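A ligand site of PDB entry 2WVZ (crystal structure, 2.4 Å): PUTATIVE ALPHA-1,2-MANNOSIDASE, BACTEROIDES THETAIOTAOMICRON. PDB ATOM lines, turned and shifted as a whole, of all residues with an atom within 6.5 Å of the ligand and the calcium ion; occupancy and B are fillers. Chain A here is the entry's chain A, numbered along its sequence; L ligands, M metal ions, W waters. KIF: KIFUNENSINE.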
ATOM      1  N   PRO A  66      -8.767 -28.038 -11.752  1.00  0.00           N
ATOM      2  CA  PRO A  66      -7.925 -26.897 -12.151  1.00  0.00           C
ATOM      3  C   PRO A  66      -8.715 -25.658 -12.680  1.00  0.00           C
ATOM      4  O   PRO A  66      -8.148 -24.573 -12.750  1.00  0.00           O
ATOM      5  CB  PRO A  66      -7.053 -27.466 -13.276  1.00  0.00           C
ATOM      6  CG  PRO A  66      -7.782 -28.702 -13.773  1.00  0.00           C
ATOM      7  CD  PRO A  66      -8.918 -29.041 -12.823  1.00  0.00           C
ATOM      8  N   SER A  67      -9.987 -25.828 -13.061  1.00  0.00           N
ATOM      9  CA  SER A  67     -10.798 -24.685 -13.530  1.00  0.00           C
ATOM     10  C   SER A  67     -12.236 -25.122 -13.671  1.00  0.00           C
ATOM     11  O   SER A  67     -12.495 -26.316 -13.883  1.00  0.00           O
ATOM     12  CB  SER A  67     -10.324 -24.189 -14.890  1.00  0.00           C
ATOM     13  OG  SER A  67     -10.720 -25.104 -15.940  1.00  0.00           O
ATOM     14  N   PRO A  68     -13.189 -24.166 -13.629  1.00  0.00           N
ATOM     15  CA  PRO A  68     -14.610 -24.494 -13.847  1.00  0.00           C
ATOM     16  C   PRO A  68     -14.845 -25.060 -15.266  1.00  0.00           C
ATOM     17  O   PRO A  68     -15.842 -25.751 -15.510  1.00  0.00           O
ATOM     18  CB  PRO A  68     -15.327 -23.152 -13.659  1.00  0.00           C
ATOM     19  CG  PRO A  68     -14.310 -22.130 -13.972  1.00  0.00           C
ATOM     20  CD  PRO A  68     -12.968 -22.705 -13.570  1.00  0.00           C
ATOM     21  N   TRP A  69     -13.900 -24.824 -16.180  1.00  0.00           N
ATOM     22  CA  TRP A  69     -14.004 -25.342 -17.550  1.00  0.00           C
ATOM     23  C   TRP A  69     -13.535 -26.785 -17.643  1.00  0.00           C
ATOM     24  O   TRP A  69     -14.215 -27.614 -18.211  1.00  0.00           O
ATOM     25  CB  TRP A  69     -13.258 -24.445 -18.538  1.00  0.00           C
ATOM     26  CG  TRP A  69     -13.555 -22.991 -18.277  1.00  0.00           C
ATOM     27  CD1 TRP A  69     -12.704 -22.057 -17.758  1.00  0.00           C
ATOM     28  CD2 TRP A  69     -14.816 -22.332 -18.456  1.00  0.00           C
ATOM     29  NE1 TRP A  69     -13.348 -20.844 -17.643  1.00  0.00           N
ATOM     30  CE2 TRP A  69     -14.644 -20.988 -18.058  1.00  0.00           C
ATOM     31  CE3 TRP A  69     -16.070 -22.737 -18.955  1.00  0.00           C
ATOM     32  CZ2 TRP A  69     -15.664 -20.049 -18.127  1.00  0.00           C
ATOM     33  CZ3 TRP A  69     -17.091 -21.799 -19.024  1.00  0.00           C
ATOM     34  CH2 TRP A  69     -16.877 -20.465 -18.611  1.00  0.00           C
ATOM     35  N   ILE A  70     -12.398 -27.101 -17.061  1.00  0.00           N
ATOM     36  CA  ILE A  70     -11.898 -28.445 -17.049  1.00  0.00           C
ATOM     37  C   ILE A  70     -12.740 -29.352 -16.152  1.00  0.00           C
ATOM     38  O   ILE A  70     -12.981 -30.508 -16.496  1.00  0.00           O
ATOM     39  CB  ILE A  70     -10.409 -28.473 -16.612  1.00  0.00           C
ATOM     40  CG1 ILE A  70      -9.555 -27.788 -17.690  1.00  0.00           C
ATOM     41  CG2 ILE A  70      -9.921 -29.877 -16.403  1.00  0.00           C
ATOM     42  CD1 ILE A  70      -9.486 -28.582 -18.996  1.00  0.00           C
ATOM     43  N   GLY A 326      -2.548 -26.600 -17.948  1.00  0.00           N
ATOM     44  CA  GLY A 326      -2.620 -26.444 -19.386  1.00  0.00           C
ATOM     45  C   GLY A 326      -1.463 -25.600 -19.861  1.00  0.00           C
ATOM     46  O   GLY A 326      -1.430 -24.425 -19.597  1.00  0.00           O
ATOM     47  N   TRP A 328      -0.760 -24.101 -22.321  1.00  0.00           N
ATOM     48  CA  TRP A 328      -1.114 -22.993 -23.182  1.00  0.00           C
ATOM     49  C   TRP A 328      -1.195 -21.745 -22.336  1.00  0.00           C
ATOM     50  O   TRP A 328      -0.888 -20.637 -22.809  1.00  0.00           O
ATOM     51  CB  TRP A 328      -2.442 -23.276 -23.895  1.00  0.00           C
ATOM     52  CG  TRP A 328      -2.937 -22.142 -24.741  1.00  0.00           C
ATOM     53  CD1 TRP A 328      -2.673 -21.933 -26.073  1.00  0.00           C
ATOM     54  CD2 TRP A 328      -3.831 -21.086 -24.349  1.00  0.00           C
ATOM     55  NE1 TRP A 328      -3.330 -20.808 -26.518  1.00  0.00           N
ATOM     56  CE2 TRP A 328      -4.044 -20.278 -25.480  1.00  0.00           C
ATOM     57  CE3 TRP A 328      -4.451 -20.744 -23.143  1.00  0.00           C
ATOM     58  CZ2 TRP A 328      -4.859 -19.129 -25.439  1.00  0.00           C
ATOM     59  CZ3 TRP A 328      -5.286 -19.615 -23.113  1.00  0.00           C
ATOM     60  CH2 TRP A 328      -5.478 -18.827 -24.246  1.00  0.00           C
ATOM     61  N   ASP A 329      -1.627 -21.923 -21.090  1.00  0.00           N
ATOM     62  CA  ASP A 329      -1.565 -20.859 -20.080  1.00  0.00           C
ATOM     63  C   ASP A 329      -0.136 -20.766 -19.544  1.00  0.00           C
ATOM     64  O   ASP A 329       0.492 -19.730 -19.659  1.00  0.00           O
ATOM     65  CB  ASP A 329      -2.464 -21.157 -18.869  1.00  0.00           C
ATOM     66  CG  ASP A 329      -3.926 -21.312 -19.227  1.00  0.00           C
ATOM     67  OD1 ASP A 329      -4.535 -22.349 -18.845  1.00  0.00           O
ATOM     68  OD2 ASP A 329      -4.463 -20.393 -19.864  1.00  0.00           O
ATOM     69  N   TRP A 366      -2.733 -30.036 -22.289  1.00  0.00           N
ATOM     70  CA  TRP A 366      -3.635 -29.926 -21.158  1.00  0.00           C
ATOM     71  C   TRP A 366      -3.750 -31.331 -20.533  1.00  0.00           C
ATOM     72  O   TRP A 366      -3.916 -32.333 -21.235  1.00  0.00           O
ATOM     73  CB  TRP A 366      -5.004 -29.411 -21.584  1.00  0.00           C
ATOM     74  CG  TRP A 366      -5.369 -28.162 -20.906  1.00  0.00           C
ATOM     75  CD1 TRP A 366      -5.549 -26.942 -21.483  1.00  0.00           C
ATOM     76  CD2 TRP A 366      -5.553 -27.967 -19.498  1.00  0.00           C
ATOM     77  NE1 TRP A 366      -5.853 -26.008 -20.528  1.00  0.00           N
ATOM     78  CE2 TRP A 366      -5.868 -26.613 -19.299  1.00  0.00           C
ATOM     79  CE3 TRP A 366      -5.489 -28.808 -18.379  1.00  0.00           C
ATOM     80  CZ2 TRP A 366      -6.115 -26.072 -18.039  1.00  0.00           C
ATOM     81  CZ3 TRP A 366      -5.727 -28.271 -17.128  1.00  0.00           C
ATOM     82  CH2 TRP A 366      -6.025 -26.911 -16.966  1.00  0.00           C
ATOM     83  N   CYS A 374      -8.367 -29.576 -24.959  1.00  0.00           N
ATOM     84  CA  CYS A 374      -8.548 -28.192 -24.545  1.00  0.00           C
ATOM     85  C   CYS A 374      -7.390 -27.321 -24.989  1.00  0.00           C
ATOM     86  O   CYS A 374      -6.256 -27.658 -24.743  1.00  0.00           O
ATOM     87  CB  CYS A 374      -8.635 -28.117 -23.015  1.00  0.00           C
ATOM     88  SG  CYS A 374      -9.041 -26.476 -22.418  1.00  0.00           S
ATOM     89  N   MET A 375      -7.700 -26.186 -25.620  1.00  0.00           N
ATOM     90  CA  MET A 375      -6.732 -25.188 -26.086  1.00  0.00           C
ATOM     91  C   MET A 375      -5.858 -25.663 -27.225  1.00  0.00           C
ATOM     92  O   MET A 375      -6.206 -26.631 -27.915  1.00  0.00           O
ATOM     93  CB  MET A 375      -5.885 -24.621 -24.948  1.00  0.00           C
ATOM     94  CG  MET A 375      -6.688 -23.999 -23.796  1.00  0.00           C
ATOM     95  SD  MET A 375      -8.258 -23.120 -24.172  1.00  0.00           S
ATOM     96  CE  MET A 375      -7.645 -21.571 -24.877  1.00  0.00           C
ATOM     97  N   GLU A 514      -9.822 -17.606 -28.585  1.00  0.00           N
ATOM     98  CA  GLU A 514     -10.299 -16.702 -27.541  1.00  0.00           C
ATOM     99  C   GLU A 514      -9.587 -15.347 -27.594  1.00  0.00           C
ATOM    100  O   GLU A 514      -9.107 -14.829 -26.574  1.00  0.00           O
ATOM    101  CB  GLU A 514     -10.160 -17.360 -26.180  1.00  0.00           C
ATOM    102  CG  GLU A 514     -10.907 -18.695 -26.035  1.00  0.00           C
ATOM    103  CD  GLU A 514     -10.588 -19.409 -24.732  1.00  0.00           C
ATOM    104  OE1 GLU A 514     -10.952 -20.603 -24.582  1.00  0.00           O
ATOM    105  OE2 GLU A 514      -9.963 -18.773 -23.843  1.00  0.00           O
ATOM    106  N   HIS A 565     -17.343 -14.619 -21.690  1.00  0.00           N
ATOM    107  CA  HIS A 565     -16.838 -13.800 -20.608  1.00  0.00           C
ATOM    108  C   HIS A 565     -15.510 -13.121 -20.952  1.00  0.00           C
ATOM    109  O   HIS A 565     -15.302 -11.998 -20.535  1.00  0.00           O
ATOM    110  CB  HIS A 565     -16.734 -14.594 -19.312  1.00  0.00           C
ATOM    111  CG  HIS A 565     -15.742 -15.695 -19.361  1.00  0.00           C
ATOM    112  ND1 HIS A 565     -14.436 -15.547 -18.938  1.00  0.00           N
ATOM    113  CD2 HIS A 565     -15.851 -16.972 -19.795  1.00  0.00           C
ATOM    114  CE1 HIS A 565     -13.790 -16.692 -19.098  1.00  0.00           C
ATOM    115  NE2 HIS A 565     -14.624 -17.567 -19.614  1.00  0.00           N
ATOM    116  N   GLU A 566     -14.627 -13.781 -21.720  1.00  0.00           N
ATOM    117  CA  GLU A 566     -13.329 -13.161 -22.111  1.00  0.00           C
ATOM    118  C   GLU A 566     -13.578 -11.882 -22.894  1.00  0.00           C
ATOM    119  O   GLU A 566     -12.846 -10.913 -22.734  1.00  0.00           O
ATOM    120  CB  GLU A 566     -12.421 -14.097 -22.921  1.00  0.00           C
ATOM    121  CG  GLU A 566     -11.827 -15.309 -22.163  1.00  0.00           C
ATOM    122  CD  GLU A 566     -12.782 -16.496 -22.128  1.00  0.00           C
ATOM    123  OE1 GLU A 566     -13.941 -16.304 -22.570  1.00  0.00           O
ATOM    124  OE2 GLU A 566     -12.377 -17.598 -21.675  1.00  0.00           O
ATOM    125  N   GLY A 581      -7.158  -9.961 -19.437  1.00  0.00           N
ATOM    126  CA  GLY A 581      -7.869 -11.122 -18.900  1.00  0.00           C
ATOM    127  C   GLY A 581      -7.580 -12.448 -19.581  1.00  0.00           C
ATOM    128  O   GLY A 581      -7.967 -13.507 -19.062  1.00  0.00           O
ATOM    129  N   ASN A 582      -6.910 -12.425 -20.736  1.00  0.00           N
ATOM    130  CA  ASN A 582      -6.582 -13.677 -21.367  1.00  0.00           C
ATOM    131  C   ASN A 582      -5.132 -13.738 -21.806  1.00  0.00           C
ATOM    132  O   ASN A 582      -4.543 -12.720 -22.201  1.00  0.00           O
ATOM    133  CB  ASN A 582      -7.570 -14.052 -22.472  1.00  0.00           C
ATOM    134  CG  ASN A 582      -7.925 -15.549 -22.463  1.00  0.00           C
ATOM    135  OD1 ASN A 582      -7.757 -16.235 -21.435  1.00  0.00           O
ATOM    136  ND2 ASN A 582      -8.423 -16.067 -23.594  1.00  0.00           N
ATOM    137  N   GLN A 583      -4.577 -14.953 -21.749  1.00  0.00           N
ATOM    138  CA  GLN A 583      -3.137 -15.205 -21.780  1.00  0.00           C
ATOM    139  C   GLN A 583      -2.392 -14.701 -22.997  1.00  0.00           C
ATOM    140  O   GLN A 583      -1.211 -14.361 -22.888  1.00  0.00           O
ATOM    141  CB  GLN A 583      -2.852 -16.706 -21.681  1.00  0.00           C
ATOM    142  CG  GLN A 583      -3.099 -17.313 -20.342  1.00  0.00           C
ATOM    143  CD  GLN A 583      -4.500 -17.061 -19.888  1.00  0.00           C
ATOM    144  OE1 GLN A 583      -5.480 -17.303 -20.612  1.00  0.00           O
ATOM    145  NE2 GLN A 583      -4.627 -16.548 -18.663  1.00  0.00           N
ATOM    146  N   PRO A 584      -3.048 -14.682 -24.166  1.00  0.00           N
ATOM    147  CA  PRO A 584      -2.252 -14.512 -25.388  1.00  0.00           C
ATOM    148  C   PRO A 584      -1.563 -13.140 -25.470  1.00  0.00           C
ATOM    149  O   PRO A 584      -0.472 -13.035 -26.000  1.00  0.00           O
ATOM    150  CB  PRO A 584      -3.264 -14.713 -26.522  1.00  0.00           C
ATOM    151  CG  PRO A 584      -4.530 -15.233 -25.868  1.00  0.00           C
ATOM    152  CD  PRO A 584      -4.494 -14.837 -24.436  1.00  0.00           C
ATOM    153  N   GLY A 622      -9.863 -11.476 -15.038  1.00  0.00           N
ATOM    154  CA  GLY A 622     -10.139 -12.640 -15.890  1.00  0.00           C
ATOM    155  C   GLY A 622      -9.764 -13.920 -15.178  1.00  0.00           C
ATOM    156  O   GLY A 622      -9.470 -13.908 -13.989  1.00  0.00           O
ATOM    157  N   ASP A 623      -9.772 -15.041 -15.884  1.00  0.00           N
ATOM    158  CA  ASP A 623      -9.454 -16.288 -15.231  1.00  0.00           C
ATOM    159  C   ASP A 623      -8.010 -16.306 -14.719  1.00  0.00           C
ATOM    160  O   ASP A 623      -7.095 -15.723 -15.312  1.00  0.00           O
ATOM    161  CB  ASP A 623      -9.706 -17.459 -16.170  1.00  0.00           C
ATOM    162  CG  ASP A 623     -11.195 -17.774 -16.347  1.00  0.00           C
ATOM    163  OD1 ASP A 623     -12.061 -16.972 -15.930  1.00  0.00           O
ATOM    164  OD2 ASP A 623     -11.507 -18.826 -16.896  1.00  0.00           O
ATOM    165  N   GLU A 624      -7.795 -16.998 -13.601  1.00  0.00           N
ATOM    166  CA  GLU A 624      -6.462 -17.090 -13.015  1.00  0.00           C
ATOM    167  C   GLU A 624      -5.555 -18.094 -13.758  1.00  0.00           C
ATOM    168  O   GLU A 624      -4.351 -17.849 -13.982  1.00  0.00           O
ATOM    169  CB  GLU A 624      -6.584 -17.475 -11.545  1.00  0.00           C
ATOM    170  CG  GLU A 624      -5.391 -17.170 -10.737  1.00  0.00           C
ATOM    171  CD  GLU A 624      -4.311 -18.188 -10.887  1.00  0.00           C
ATOM    172  OE1 GLU A 624      -4.650 -19.388 -10.959  1.00  0.00           O
ATOM    173  OE2 GLU A 624      -3.124 -17.798 -10.926  1.00  0.00           O
ATOM    174  N   ASP A 625      -6.149 -19.228 -14.098  1.00  0.00           N
ATOM    175  CA  ASP A 625      -5.527 -20.250 -14.911  1.00  0.00           C
ATOM    176  C   ASP A 625      -4.237 -20.780 -14.340  1.00  0.00           C
ATOM    177  O   ASP A 625      -3.173 -20.680 -14.966  1.00  0.00           O
ATOM    178  CB  ASP A 625      -5.309 -19.752 -16.329  1.00  0.00           C
ATOM    179  CG  ASP A 625      -6.613 -19.495 -17.065  1.00  0.00           C
ATOM    180  OD1 ASP A 625      -7.595 -20.290 -16.912  1.00  0.00           O
ATOM    181  OD2 ASP A 625      -6.661 -18.490 -17.809  1.00  0.00           O
ATOM    182  N   ASN A 626      -4.346 -21.359 -13.154  1.00  0.00           N
ATOM    183  CA  ASN A 626      -3.308 -22.236 -12.623  1.00  0.00           C
ATOM    184  C   ASN A 626      -1.925 -21.660 -12.438  1.00  0.00           C
ATOM    185  O   ASN A 626      -0.921 -22.379 -12.533  1.00  0.00           O
ATOM    186  CB  ASN A 626      -3.285 -23.493 -13.452  1.00  0.00           C
ATOM    187  CG  ASN A 626      -4.666 -24.056 -13.610  1.00  0.00           C
ATOM    188  OD1 ASN A 626      -5.144 -24.233 -14.711  1.00  0.00           O
ATOM    189  ND2 ASN A 626      -5.336 -24.277 -12.492  1.00  0.00           N
ATOM    190  N   THR A 629      -1.952 -16.064 -14.638  1.00  0.00           N
ATOM    191  CA  THR A 629      -2.374 -14.676 -14.507  1.00  0.00           C
ATOM    192  C   THR A 629      -1.801 -14.051 -13.220  1.00  0.00           C
ATOM    193  O   THR A 629      -1.613 -12.820 -13.124  1.00  0.00           O
ATOM    194  CB  THR A 629      -3.905 -14.635 -14.524  1.00  0.00           C
ATOM    195  OG1 THR A 629      -4.358 -15.298 -15.708  1.00  0.00           O
ATOM    196  CG2 THR A 629      -4.437 -13.200 -14.479  1.00  0.00           C
HETATM  197  C4  KIF L   1      -7.721 -22.449 -19.946  1.00  0.00           C
HETATM  198  O4  KIF L   1      -6.528 -23.186 -20.094  1.00  0.00           O
HETATM  199  C3  KIF L   1      -7.646 -21.188 -20.855  1.00  0.00           C
HETATM  200  O3  KIF L   1      -6.973 -20.105 -20.157  1.00  0.00           O
HETATM  201  C2  KIF L   1      -9.055 -20.747 -21.332  1.00  0.00           C
HETATM  202  O2  KIF L   1      -9.092 -19.341 -21.561  1.00  0.00           O
HETATM  203  C1  KIF L   1     -10.130 -21.190 -20.333  1.00  0.00           C
HETATM  204  N9  KIF L   1     -11.489 -20.737 -20.796  1.00  0.00           N
HETATM  205  C8  KIF L   1     -12.121 -21.796 -21.341  1.00  0.00           C
HETATM  206  O8  KIF L   1     -13.251 -21.812 -21.848  1.00  0.00           O
HETATM  207  C7  KIF L   1     -11.316 -22.937 -21.229  1.00  0.00           C
HETATM  208  O7  KIF L   1     -11.637 -24.044 -21.661  1.00  0.00           O
HETATM  209  N   KIF L   1     -10.122 -22.635 -20.542  1.00  0.00           N
HETATM  210  C5  KIF L   1      -8.890 -23.400 -20.299  1.00  0.00           C
HETATM  211  C6  KIF L   1      -9.107 -24.483 -19.250  1.00  0.00           C
HETATM  212  O6  KIF L   1      -9.467 -23.818 -18.057  1.00  0.00           O
HETATM  213 CA    CA M   1      -8.011 -17.860 -19.981  1.00  0.00          CA
HETATM  214  O   HOH W   1     -10.371 -16.872 -19.498  1.00  0.00           O
HETATM  215  O   HOH W   2      -7.309 -16.096 -18.248  1.00  0.00           O
HETATM  216  O   HOH W   3      -7.348 -22.947 -16.561  1.00  0.00           O
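Residues that only touch the ligand: Trp 69 (3.5 Å), Ile 70 (3.7 Å), Trp 328 (3.4 Å) and Met 375 (3.8 Å). Hydrophobic or aromatic side chains within 4 Å of the ligand: Trp 69, Ile 70, Trp 328, Trp 366 and Met 375. Within 4 Å of the ligand: Ser 67, Trp 69, Ile 70, Trp 328, Asp 329, Trp 366, Cys 374, Met 375, Glu 514, Glu 566, Asn 582, Gln 583 and Asp 625.
The indole nitrogen of Trp 69 lies within hydrogen-bond range of the side-chain carboxylate of Asp 623. The backbone NH (N) of Trp 69 sits close to the side-chain hydroxyl (OG) of Ser 67, 3.2 Å away. The side-chain hydroxyl (OG) of Ser 67 lies within hydrogen-bond range of the backbone NH (N) of Ile 70. NE1 of Trp 366 lies close to SG of Cys 374 (3.7 Å). A ring nitrogen (NE2) of His 565 is in hydrogen-bond range of the side-chain carboxylate (OE2) of Glu 566, 3.0 Å away. The side-chain amide nitrogen (NE2) of Gln 583 sits at hydrogen-bond distance from the side-chain hydroxyl (OG1) of Thr 629, 3.2 Å away. OE2 of Glu 514 is in hydrogen-bond range of ND2 of Asn 582, at 3.1 Å. OE1 of Gln 583 lies close to OD2 of Asp 329.
Of the 24 residues printed, 3 come within 4 Å of the calcium ion.
OE2 of Glu 514 lies close to O2 of the ligand. OD1 of Asp 329 is in hydrogen-bond range of O4 of the ligand, 2.5 Å away. An oxygen (O4) of the ligand sits at hydrogen-bond distance from the indole nitrogen (NE1) of Trp 366. The side-chain carboxylate (OE2) of Glu 566 is in hydrogen-bond range of a nitrogen (N9) of the ligand, 3.4 Å away. SG of Cys 374 is in hydrogen-bond range of O7 of the ligand (3.6 Å). The side-chain hydroxyl of Ser 67 is in hydrogen-bond range of an oxygen (O6) of the ligand, at 2.8 Å.
The calcium ion is bound by the side-chain amide oxygen of Asn 582, an oxygen (O2) of the ligand, an oxygen (O3) of the ligand, water W2, water W1, the side-chain carboxylate of Asp 625 and the side-chain amide oxygen of Gln 583. The calcium ion has seven donor atoms within binding distance.
Water W2 lies within hydrogen-bond range of the side-chain amide nitrogen of Gln 583 (2.8 Å), the backbone carbonyl oxygen of Gly 581 (2.8 Å) and the backbone carbonyl oxygen of Asp 623 (3.0 Å). Water W1 lies within hydrogen-bond range of the side-chain carboxylate (OE2) of Glu 566 and the side-chain carboxylate (OD2) of Asp 623. Water W3 lies within hydrogen-bond range of OD1 of Asp 625 (2.7 Å), O6 of the ligand (2.7 Å) and OD1 of Asn 626 (3.2 Å).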
